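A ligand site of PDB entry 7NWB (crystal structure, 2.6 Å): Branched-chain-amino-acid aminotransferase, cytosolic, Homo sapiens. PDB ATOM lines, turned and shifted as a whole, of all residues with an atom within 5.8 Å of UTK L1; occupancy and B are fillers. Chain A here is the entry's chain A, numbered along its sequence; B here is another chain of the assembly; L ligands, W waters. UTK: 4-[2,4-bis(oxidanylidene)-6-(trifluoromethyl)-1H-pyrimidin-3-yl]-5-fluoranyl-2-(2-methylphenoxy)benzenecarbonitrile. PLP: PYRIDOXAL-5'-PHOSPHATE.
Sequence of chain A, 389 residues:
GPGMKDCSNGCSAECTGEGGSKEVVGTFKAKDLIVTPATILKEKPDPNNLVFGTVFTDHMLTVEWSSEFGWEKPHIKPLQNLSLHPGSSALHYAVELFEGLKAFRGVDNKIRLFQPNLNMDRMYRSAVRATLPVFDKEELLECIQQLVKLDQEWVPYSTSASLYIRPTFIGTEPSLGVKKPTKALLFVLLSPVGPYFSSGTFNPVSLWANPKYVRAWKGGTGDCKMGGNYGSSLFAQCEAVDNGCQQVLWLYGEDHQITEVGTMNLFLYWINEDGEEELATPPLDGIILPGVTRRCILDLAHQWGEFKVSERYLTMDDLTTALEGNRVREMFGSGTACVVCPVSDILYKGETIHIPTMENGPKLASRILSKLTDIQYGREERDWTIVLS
OH of Tyr 196 sits at hydrogen-bond distance from O10 of UTK L1. A nitrogen (N9) of UTK L1 lies close to the side-chain amide nitrogen of Gln 247 (3.2 Å). The backbone NH (N) of Val 178 of chain B lies within hydrogen-bond range of an oxygen (O8) of UTK L1, at 2.8 Å. OH of Tyr 230 sits at hydrogen-bond distance from O3 of PLP L2, 2.4 Å away. N of Thr 336 lies within hydrogen-bond range of O2P of PLP L2, 2.7 Å away. The side-chain amino group of Lys 225 is covalently linked to a carbon (C4A) of PLP L2. The side-chain hydroxyl (OG1) of Thr 336 lies within hydrogen-bond range of an oxygen (O2P) of PLP L2, at 2.9 Å.
The side-chain amino group of Lys 102 sits at hydrogen-bond distance from the backbone carbonyl oxygen of Thr 336 (3.1 Å). OH of Tyr 164 is in hydrogen-bond range of NH2 of Arg 166, at 2.9 Å. The backbone carbonyl oxygen (O) of Ala 337 lies within hydrogen-bond range of the side-chain amino group (NZ) of Lys 102, at 3.4 Å. The backbone NH (N) of Phe 98 lies within hydrogen-bond range of the backbone carbonyl oxygen (O) of Lys 225 (3.1 Å). The side-chain hydroxyl of Tyr 196 lies within hydrogen-bond range of the side-chain amide nitrogen of Gln 247 (3.3 Å). OH of Tyr 93 of chain B sits at hydrogen-bond distance from NH1 of Arg 166, at 2.9 Å. The side-chain amide nitrogen of Gln 237 lies within hydrogen-bond range of the backbone carbonyl oxygen of Gln 246 (3.2 Å). O of Leu 176 of chain B is in hydrogen-bond range of OH of Tyr 93 of chain B (2.5 Å).
The side-chain amide oxygen (OE1) of Gln 237 sits close to a fluorine (F20) of UTK L1. Phe 52 touches UTK L1 (CE1 to C18, 3.1 Å). Phe 98 touches UTK L1. Lys 102 touches UTK L1 (CE to N23, 3.9 Å). Tyr 164 touches UTK L1. Arg 166 touches UTK L1 (NH2 to C27, 3.5 Å). NZ of Lys 225 touches C28 of UTK L1 (3.8 Å). Gln 246 touches UTK L1. CB of Thr 263 touches C28 of UTK L1 (3.5 Å). Ala 337 touches UTK L1. OH of Tyr 93 of chain B touches C27 of UTK L1, 3.3 Å away. O of Leu 176 of chain B touches C27 of UTK L1 (3.6 Å). Gly 177 of chain B touches UTK L1 (CA to O8, 3.6 Å). Within 4 Å of UTK L1: Phe 52, Phe 98, Lys 102, Tyr 164, Arg 166, Tyr 196, Lys 225, Gln 237, Gln 246, Gln 247, Thr 263, Ala 337, Tyr 93 of chain B, Leu 176 of chain B, Gly 177 of chain B and Val 178 of chain B.
Water W1 lies within hydrogen-bond range of the side-chain hydroxyl (OG1) of Thr 263 and an oxygen (O10) of UTK L1.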
ATOM      1  N   PHE A  52     -13.821  16.160   8.415  1.00  0.00           N
ATOM      2  CA  PHE A  52     -12.839  16.090   9.520  1.00  0.00           C
ATOM      3  C   PHE A  52     -12.202  17.470   9.777  1.00  0.00           C
ATOM      4  O   PHE A  52     -11.715  18.063   8.819  1.00  0.00           O
ATOM      5  CB  PHE A  52     -11.747  15.056   9.285  1.00  0.00           C
ATOM      6  CG  PHE A  52     -10.752  15.077  10.404  1.00  0.00           C
ATOM      7  CD1 PHE A  52     -11.072  14.495  11.629  1.00  0.00           C
ATOM      8  CD2 PHE A  52      -9.557  15.751  10.278  1.00  0.00           C
ATOM      9  CE1 PHE A  52     -10.185  14.565  12.691  1.00  0.00           C
ATOM     10  CE2 PHE A  52      -8.657  15.791  11.337  1.00  0.00           C
ATOM     11  CZ  PHE A  52      -8.979  15.200  12.541  1.00  0.00           C
ATOM     12  N   PHE A  98       1.243  18.320  19.257  1.00  0.00           N
ATOM     13  CA  PHE A  98      -0.209  18.127  19.347  1.00  0.00           C
ATOM     14  C   PHE A  98      -0.516  16.686  19.760  1.00  0.00           C
ATOM     15  O   PHE A  98       0.374  15.811  19.745  1.00  0.00           O
ATOM     16  CB  PHE A  98      -0.863  18.484  18.014  1.00  0.00           C
ATOM     17  CG  PHE A  98      -0.494  17.565  16.882  1.00  0.00           C
ATOM     18  CD1 PHE A  98       0.698  17.708  16.204  1.00  0.00           C
ATOM     19  CD2 PHE A  98      -1.355  16.541  16.499  1.00  0.00           C
ATOM     20  CE1 PHE A  98       1.037  16.852  15.174  1.00  0.00           C
ATOM     21  CE2 PHE A  98      -1.012  15.695  15.460  1.00  0.00           C
ATOM     22  CZ  PHE A  98       0.173  15.850  14.791  1.00  0.00           C
ATOM     23  N   LYS A 102     -10.415  11.034  20.965  1.00  0.00           N
ATOM     24  CA  LYS A 102     -11.857  11.256  20.680  1.00  0.00           C
ATOM     25  C   LYS A 102     -12.678  11.029  21.962  1.00  0.00           C
ATOM     26  O   LYS A 102     -12.233  10.270  22.836  1.00  0.00           O
ATOM     27  CB  LYS A 102     -12.303  10.366  19.522  1.00  0.00           C
ATOM     28  CG  LYS A 102     -11.783  10.810  18.161  1.00  0.00           C
ATOM     29  CD  LYS A 102     -12.119   9.858  17.026  1.00  0.00           C
ATOM     30  CE  LYS A 102     -11.917  10.500  15.663  1.00  0.00           C
ATOM     31  NZ  LYS A 102     -12.192   9.584  14.532  1.00  0.00           N
ATOM     32  N   TYR A 164     -13.566  15.128  18.199  1.00  0.00           N
ATOM     33  CA  TYR A 164     -12.087  15.130  18.121  1.00  0.00           C
ATOM     34  C   TYR A 164     -11.566  16.176  19.113  1.00  0.00           C
ATOM     35  O   TYR A 164     -12.024  17.336  19.078  1.00  0.00           O
ATOM     36  CB  TYR A 164     -11.588  15.384  16.707  1.00  0.00           C
ATOM     37  CG  TYR A 164     -10.107  15.164  16.499  1.00  0.00           C
ATOM     38  CD1 TYR A 164      -9.563  13.898  16.588  1.00  0.00           C
ATOM     39  CD2 TYR A 164      -9.252  16.206  16.192  1.00  0.00           C
ATOM     40  CE1 TYR A 164      -8.214  13.666  16.367  1.00  0.00           C
ATOM     41  CE2 TYR A 164      -7.901  16.001  15.978  1.00  0.00           C
ATOM     42  CZ  TYR A 164      -7.383  14.725  16.064  1.00  0.00           C
ATOM     43  OH  TYR A 164      -6.054  14.500  15.851  1.00  0.00           O
ATOM     44  N   ARG A 166      -8.190  18.030  20.253  1.00  0.00           N
ATOM     45  CA  ARG A 166      -6.868  18.446  19.705  1.00  0.00           C
ATOM     46  C   ARG A 166      -6.145  19.275  20.760  1.00  0.00           C
ATOM     47  O   ARG A 166      -6.209  20.504  20.747  1.00  0.00           O
ATOM     48  CB  ARG A 166      -7.063  19.206  18.391  1.00  0.00           C
ATOM     49  CG  ARG A 166      -5.829  19.933  17.848  1.00  0.00           C
ATOM     50  CD  ARG A 166      -4.560  19.113  17.833  1.00  0.00           C
ATOM     51  NE  ARG A 166      -4.656  17.954  16.950  1.00  0.00           N
ATOM     52  CZ  ARG A 166      -4.413  17.947  15.644  1.00  0.00           C
ATOM     53  NH1 ARG A 166      -4.028  19.047  15.021  1.00  0.00           N
ATOM     54  NH2 ARG A 166      -4.556  16.826  14.958  1.00  0.00           N
ATOM     55  N   VAL A 193     -16.558  15.281  14.417  1.00  0.00           N
ATOM     56  CA  VAL A 193     -16.171  14.590  13.152  1.00  0.00           C
ATOM     57  C   VAL A 193     -17.042  13.356  12.968  1.00  0.00           C
ATOM     58  O   VAL A 193     -17.396  12.729  13.970  1.00  0.00           O
ATOM     59  CB  VAL A 193     -14.679  14.207  13.127  1.00  0.00           C
ATOM     60  CG1 VAL A 193     -13.807  15.423  13.378  1.00  0.00           C
ATOM     61  CG2 VAL A 193     -14.327  13.084  14.097  1.00  0.00           C
ATOM     62  N   TYR A 196     -14.895   8.057   9.339  1.00  0.00           N
ATOM     63  CA  TYR A 196     -13.696   8.332   8.500  1.00  0.00           C
ATOM     64  C   TYR A 196     -14.103   8.371   7.021  1.00  0.00           C
ATOM     65  O   TYR A 196     -13.727   9.332   6.317  1.00  0.00           O
ATOM     66  CB  TYR A 196     -12.592   7.297   8.709  1.00  0.00           C
ATOM     67  CG  TYR A 196     -11.299   7.641   8.009  1.00  0.00           C
ATOM     68  CD1 TYR A 196     -10.514   8.713   8.412  1.00  0.00           C
ATOM     69  CD2 TYR A 196     -10.855   6.877   6.931  1.00  0.00           C
ATOM     70  CE1 TYR A 196      -9.333   9.020   7.756  1.00  0.00           C
ATOM     71  CE2 TYR A 196      -9.659   7.162   6.294  1.00  0.00           C
ATOM     72  CZ  TYR A 196      -8.891   8.233   6.708  1.00  0.00           C
ATOM     73  OH  TYR A 196      -7.706   8.491   6.069  1.00  0.00           O
ATOM     74  N   LYS A 225       4.718  13.314  18.386  1.00  0.00           N
ATOM     75  CA  LYS A 225       3.716  14.091  17.636  1.00  0.00           C
ATOM     76  C   LYS A 225       4.153  15.560  17.680  1.00  0.00           C
ATOM     77  O   LYS A 225       3.371  16.407  18.148  1.00  0.00           O
ATOM     78  CB  LYS A 225       2.291  13.814  18.146  1.00  0.00           C
ATOM     79  CG  LYS A 225       1.501  12.865  17.256  1.00  0.00           C
ATOM     80  CD  LYS A 225       0.120  12.512  17.733  1.00  0.00           C
ATOM     81  CE  LYS A 225      -0.794  12.112  16.590  1.00  0.00           C
ATOM     82  NZ  LYS A 225      -0.297  10.916  15.871  1.00  0.00           N
ATOM     83  N   TYR A 230       5.308  16.591  10.301  1.00  0.00           N
ATOM     84  CA  TYR A 230       4.103  16.562   9.421  1.00  0.00           C
ATOM     85  C   TYR A 230       4.283  17.531   8.241  1.00  0.00           C
ATOM     86  O   TYR A 230       3.876  17.147   7.135  1.00  0.00           O
ATOM     87  CB  TYR A 230       2.839  16.703  10.276  1.00  0.00           C
ATOM     88  CG  TYR A 230       2.790  15.612  11.313  1.00  0.00           C
ATOM     89  CD1 TYR A 230       2.321  14.337  11.012  1.00  0.00           C
ATOM     90  CD2 TYR A 230       3.376  15.817  12.541  1.00  0.00           C
ATOM     91  CE1 TYR A 230       2.361  13.319  11.942  1.00  0.00           C
ATOM     92  CE2 TYR A 230       3.429  14.799  13.489  1.00  0.00           C
ATOM     93  CZ  TYR A 230       2.929  13.544  13.182  1.00  0.00           C
ATOM     94  OH  TYR A 230       3.029  12.579  14.133  1.00  0.00           O
ATOM     95  N   GLN A 237       2.260  13.733  -0.069  1.00  0.00           N
ATOM     96  CA  GLN A 237       0.804  13.447  -0.065  1.00  0.00           C
ATOM     97  C   GLN A 237       0.197  13.942  -1.384  1.00  0.00           C
ATOM     98  O   GLN A 237      -0.575  13.197  -1.983  1.00  0.00           O
ATOM     99  CB  GLN A 237       0.122  14.077   1.162  1.00  0.00           C
ATOM    100  CG  GLN A 237      -1.379  13.790   1.292  1.00  0.00           C
ATOM    101  CD  GLN A 237      -1.770  12.345   1.093  1.00  0.00           C
ATOM    102  OE1 GLN A 237      -1.163  11.398   1.600  1.00  0.00           O
ATOM    103  NE2 GLN A 237      -2.844  12.142   0.337  1.00  0.00           N
ATOM    104  N   GLN A 246      -4.389   7.496  -2.164  1.00  0.00           N
ATOM    105  CA  GLN A 246      -5.092   8.211  -1.075  1.00  0.00           C
ATOM    106  C   GLN A 246      -4.127   8.489   0.087  1.00  0.00           C
ATOM    107  O   GLN A 246      -4.422   9.419   0.861  1.00  0.00           O
ATOM    108  CB  GLN A 246      -6.284   7.380  -0.573  1.00  0.00           C
ATOM    109  CG  GLN A 246      -7.471   7.345  -1.514  1.00  0.00           C
ATOM    110  CD  GLN A 246      -7.246   6.432  -2.691  1.00  0.00           C
ATOM    111  OE1 GLN A 246      -6.955   5.252  -2.546  1.00  0.00           O
ATOM    112  NE2 GLN A 246      -7.372   6.981  -3.885  1.00  0.00           N
ATOM    113  N   GLN A 247      -3.055   7.690   0.230  1.00  0.00           N
ATOM    114  CA  GLN A 247      -2.052   7.807   1.322  1.00  0.00           C
ATOM    115  C   GLN A 247      -0.645   7.480   0.810  1.00  0.00           C
ATOM    116  O   GLN A 247      -0.519   6.854  -0.243  1.00  0.00           O
ATOM    117  CB  GLN A 247      -2.368   6.845   2.451  1.00  0.00           C
ATOM    118  CG  GLN A 247      -3.711   7.089   3.126  1.00  0.00           C
ATOM    119  CD  GLN A 247      -3.742   8.341   3.965  1.00  0.00           C
ATOM    120  OE1 GLN A 247      -2.721   8.881   4.384  1.00  0.00           O
ATOM    121  NE2 GLN A 247      -4.952   8.786   4.269  1.00  0.00           N
ATOM    122  N   THR A 263      -0.362   8.970   8.179  1.00  0.00           N
ATOM    123  CA  THR A 263      -0.322   9.250   9.637  1.00  0.00           C
ATOM    124  C   THR A 263      -1.015   8.108  10.396  1.00  0.00           C
ATOM    125  O   THR A 263      -1.671   8.388  11.440  1.00  0.00           O
ATOM    126  CB  THR A 263      -0.902  10.647   9.910  1.00  0.00           C
ATOM    127  OG1 THR A 263      -2.234  10.728   9.399  1.00  0.00           O
ATOM    128  CG2 THR A 263      -0.079  11.740   9.275  1.00  0.00           C
ATOM    129  N   MET A 264      -0.875   6.879   9.880  1.00  0.00           N
ATOM    130  CA  MET A 264      -1.432   5.629  10.469  1.00  0.00           C
ATOM    131  C   MET A 264      -0.318   4.592  10.605  1.00  0.00           C
ATOM    132  O   MET A 264       0.549   4.521   9.707  1.00  0.00           O
ATOM    133  CB  MET A 264      -2.527   5.045   9.582  1.00  0.00           C
ATOM    134  CG  MET A 264      -3.805   5.857   9.498  1.00  0.00           C
ATOM    135  SD  MET A 264      -4.941   5.142   8.299  1.00  0.00           S
ATOM    136  CE  MET A 264      -4.375   5.942   6.810  1.00  0.00           C
ATOM    137  N   THR A 336      -6.401   6.737  15.413  1.00  0.00           N
ATOM    138  CA  THR A 336      -7.612   7.357  16.012  1.00  0.00           C
ATOM    139  C   THR A 336      -8.554   7.759  14.868  1.00  0.00           C
ATOM    140  O   THR A 336      -9.785   7.691  15.058  1.00  0.00           O
ATOM    141  CB  THR A 336      -7.213   8.524  16.937  1.00  0.00           C
ATOM    142  OG1 THR A 336      -6.643   7.987  18.131  1.00  0.00           O
ATOM    143  CG2 THR A 336      -8.384   9.415  17.318  1.00  0.00           C
ATOM    144  N   ALA A 337      -7.989   8.163  13.735  1.00  0.00           N
ATOM    145  CA  ALA A 337      -8.717   8.704  12.562  1.00  0.00           C
ATOM    146  C   ALA A 337      -9.674   7.651  12.028  1.00  0.00           C
ATOM    147  O   ALA A 337     -10.868   7.896  11.933  1.00  0.00           O
ATOM    148  CB  ALA A 337      -7.737   9.099  11.489  1.00  0.00           C
ATOM    149  N   CYS A 338      -9.091   6.521  11.674  1.00  0.00           N
ATOM    150  CA  CYS A 338      -9.713   5.381  10.975  1.00  0.00           C
ATOM    151  C   CYS A 338      -9.191   4.133  11.669  1.00  0.00           C
ATOM    152  O   CYS A 338      -8.032   3.751  11.371  1.00  0.00           O
ATOM    153  CB  CYS A 338      -9.294   5.382   9.520  1.00  0.00           C
ATOM    154  SG  CYS A 338      -9.542   3.778   8.728  1.00  0.00           S
ATOM    155  N   TYR B  93       1.168  21.371  12.103  1.00  0.00           N
ATOM    156  CA  TYR B  93       1.933  20.528  11.151  1.00  0.00           C
ATOM    157  C   TYR B  93       3.119  21.320  10.584  1.00  0.00           C
ATOM    158  O   TYR B  93       3.647  20.907   9.534  1.00  0.00           O
ATOM    159  CB  TYR B  93       1.020  20.007  10.047  1.00  0.00           C
ATOM    160  CG  TYR B  93      -0.286  19.502  10.588  1.00  0.00           C
ATOM    161  CD1 TYR B  93      -0.299  18.510  11.550  1.00  0.00           C
ATOM    162  CD2 TYR B  93      -1.491  20.046  10.194  1.00  0.00           C
ATOM    163  CE1 TYR B  93      -1.482  18.056  12.098  1.00  0.00           C
ATOM    164  CE2 TYR B  93      -2.694  19.595  10.713  1.00  0.00           C
ATOM    165  CZ  TYR B  93      -2.686  18.605  11.687  1.00  0.00           C
ATOM    166  OH  TYR B  93      -3.849  18.143  12.228  1.00  0.00           O
ATOM    167  N   LEU B 176      -7.976  21.226  10.733  1.00  0.00           N
ATOM    168  CA  LEU B 176      -7.038  20.265  11.372  1.00  0.00           C
ATOM    169  C   LEU B 176      -6.638  19.191  10.363  1.00  0.00           C
ATOM    170  O   LEU B 176      -5.760  18.400  10.685  1.00  0.00           O
ATOM    171  CB  LEU B 176      -7.716  19.635  12.591  1.00  0.00           C
ATOM    172  CG  LEU B 176      -8.169  20.596  13.682  1.00  0.00           C
ATOM    173  CD1 LEU B 176      -8.539  19.798  14.930  1.00  0.00           C
ATOM    174  CD2 LEU B 176      -7.102  21.653  13.976  1.00  0.00           C
ATOM    175  N   GLY B 177      -7.296  19.150   9.212  1.00  0.00           N
ATOM    176  CA  GLY B 177      -6.906  18.269   8.097  1.00  0.00           C
ATOM    177  C   GLY B 177      -5.447  18.497   7.746  1.00  0.00           C
ATOM    178  O   GLY B 177      -5.030  19.692   7.641  1.00  0.00           O
ATOM    179  N   VAL B 178      -4.702  17.404   7.588  1.00  0.00           N
ATOM    180  CA  VAL B 178      -3.280  17.424   7.125  1.00  0.00           C
ATOM    181  C   VAL B 178      -3.324  17.549   5.595  1.00  0.00           C
ATOM    182  O   VAL B 178      -3.465  16.526   4.924  1.00  0.00           O
ATOM    183  CB  VAL B 178      -2.469  16.195   7.588  1.00  0.00           C
ATOM    184  CG1 VAL B 178      -1.015  16.275   7.160  1.00  0.00           C
ATOM    185  CG2 VAL B 178      -2.535  16.008   9.095  1.00  0.00           C
ATOM    186  N   LYS B 179      -3.217  18.781   5.084  1.00  0.00           N
ATOM    187  CA  LYS B 179      -3.329  19.060   3.633  1.00  0.00           C
ATOM    188  C   LYS B 179      -2.567  20.351   3.265  1.00  0.00           C
ATOM    189  O   LYS B 179      -2.309  21.187   4.158  1.00  0.00           O
ATOM    190  CB  LYS B 179      -4.807  19.190   3.269  1.00  0.00           C
ATOM    191  CG  LYS B 179      -5.463  20.515   3.666  1.00  0.00           C
ATOM    192  CD  LYS B 179      -6.603  20.480   4.704  1.00  0.00           C
ATOM    193  CE  LYS B 179      -7.936  21.073   4.241  1.00  0.00           C
ATOM    194  NZ  LYS B 179      -9.079  20.339   4.824  1.00  0.00           N
HETATM  195  N1  UTK L   1      -6.018  12.566   7.838  1.00  0.00           N
HETATM  196  C4  UTK L   1      -5.892  11.415   7.075  1.00  0.00           C
HETATM  197  C5  UTK L   1      -5.681  12.397  10.229  1.00  0.00           C
HETATM  198  C6  UTK L   1      -7.928  12.376   9.229  1.00  0.00           C
HETATM  199  C7  UTK L   1      -5.214  13.916   5.980  1.00  0.00           C
HETATM  200  C15 UTK L   1      -7.727  12.204  11.602  1.00  0.00           C
HETATM  201  C17 UTK L   1      -4.562  12.767   3.773  1.00  0.00           C
HETATM  202  C24 UTK L   1      -4.067  14.116  12.270  1.00  0.00           C
HETATM  203  C26 UTK L   1      -2.775  14.572  12.250  1.00  0.00           C
HETATM  204  C28 UTK L   1      -1.991  12.356  12.818  1.00  0.00           C
HETATM  205  C27 UTK L   1      -5.162  15.117  11.968  1.00  0.00           C
HETATM  206  C29 UTK L   1      -1.747  13.696  12.528  1.00  0.00           C
HETATM  207  C25 UTK L   1      -3.271  11.896  12.820  1.00  0.00           C
HETATM  208  C19 UTK L   1      -4.308  12.772  12.548  1.00  0.00           C
HETATM  209  O16 UTK L   1      -5.544  12.248  12.603  1.00  0.00           O
HETATM  210  C11 UTK L   1      -6.304  12.278  11.473  1.00  0.00           C
HETATM  211  C18 UTK L   1      -8.291  12.076  12.909  1.00  0.00           C
HETATM  212  N23 UTK L   1      -8.738  11.993  13.957  1.00  0.00           N
HETATM  213  C12 UTK L   1      -8.551  12.257  10.472  1.00  0.00           C
HETATM  214  F13 UTK L   1      -8.711  12.417   8.120  1.00  0.00           F
HETATM  215  C2  UTK L   1      -6.521  12.448   9.111  1.00  0.00           C
HETATM  216  C3  UTK L   1      -5.690  13.814   7.293  1.00  0.00           C
HETATM  217  O8  UTK L   1      -5.811  14.826   7.993  1.00  0.00           O
HETATM  218  C14 UTK L   1      -5.077  12.758   5.215  1.00  0.00           C
HETATM  219  F21 UTK L   1      -4.232  13.994   3.432  1.00  0.00           F
HETATM  220  F22 UTK L   1      -5.521  12.332   2.957  1.00  0.00           F
HETATM  221  F20 UTK L   1      -3.506  11.988   3.640  1.00  0.00           F
HETATM  222  N9  UTK L   1      -5.419  11.541   5.762  1.00  0.00           N
HETATM  223  O10 UTK L   1      -6.176  10.317   7.548  1.00  0.00           O
HETATM  224  N1  PLP L   2       1.586   7.531  12.814  1.00  0.00           N
HETATM  225  C2  PLP L   2       1.814   8.842  12.923  1.00  0.00           C
HETATM  226  C2A PLP L   2       2.920   9.445  12.135  1.00  0.00           C
HETATM  227  C3  PLP L   2       1.018   9.625  13.756  1.00  0.00           C
HETATM  228  O3  PLP L   2       1.282  10.948  13.833  1.00  0.00           O
HETATM  229  C4  PLP L   2      -0.037   9.022  14.495  1.00  0.00           C
HETATM  230  C4A PLP L   2      -0.853   9.879  15.362  1.00  0.00           C
HETATM  231  C5  PLP L   2      -0.243   7.632  14.370  1.00  0.00           C
HETATM  232  C6  PLP L   2       0.590   6.947  13.516  1.00  0.00           C
HETATM  233  C5A PLP L   2      -1.340   6.869  15.064  1.00  0.00           C
HETATM  234  O4P PLP L   2      -1.729   7.393  16.373  1.00  0.00           O
HETATM  235  P   PLP L   2      -3.049   6.902  17.188  1.00  0.00           P
HETATM  236  O1P PLP L   2      -2.710   7.221  18.654  1.00  0.00           O
HETATM  237  O2P PLP L   2      -4.200   7.722  16.631  1.00  0.00           O
HETATM  238  O3P PLP L   2      -3.216   5.404  16.983  1.00  0.00           O
HETATM  239  O   HOH W   1      -4.559   9.011   9.811  1.00  0.00           O
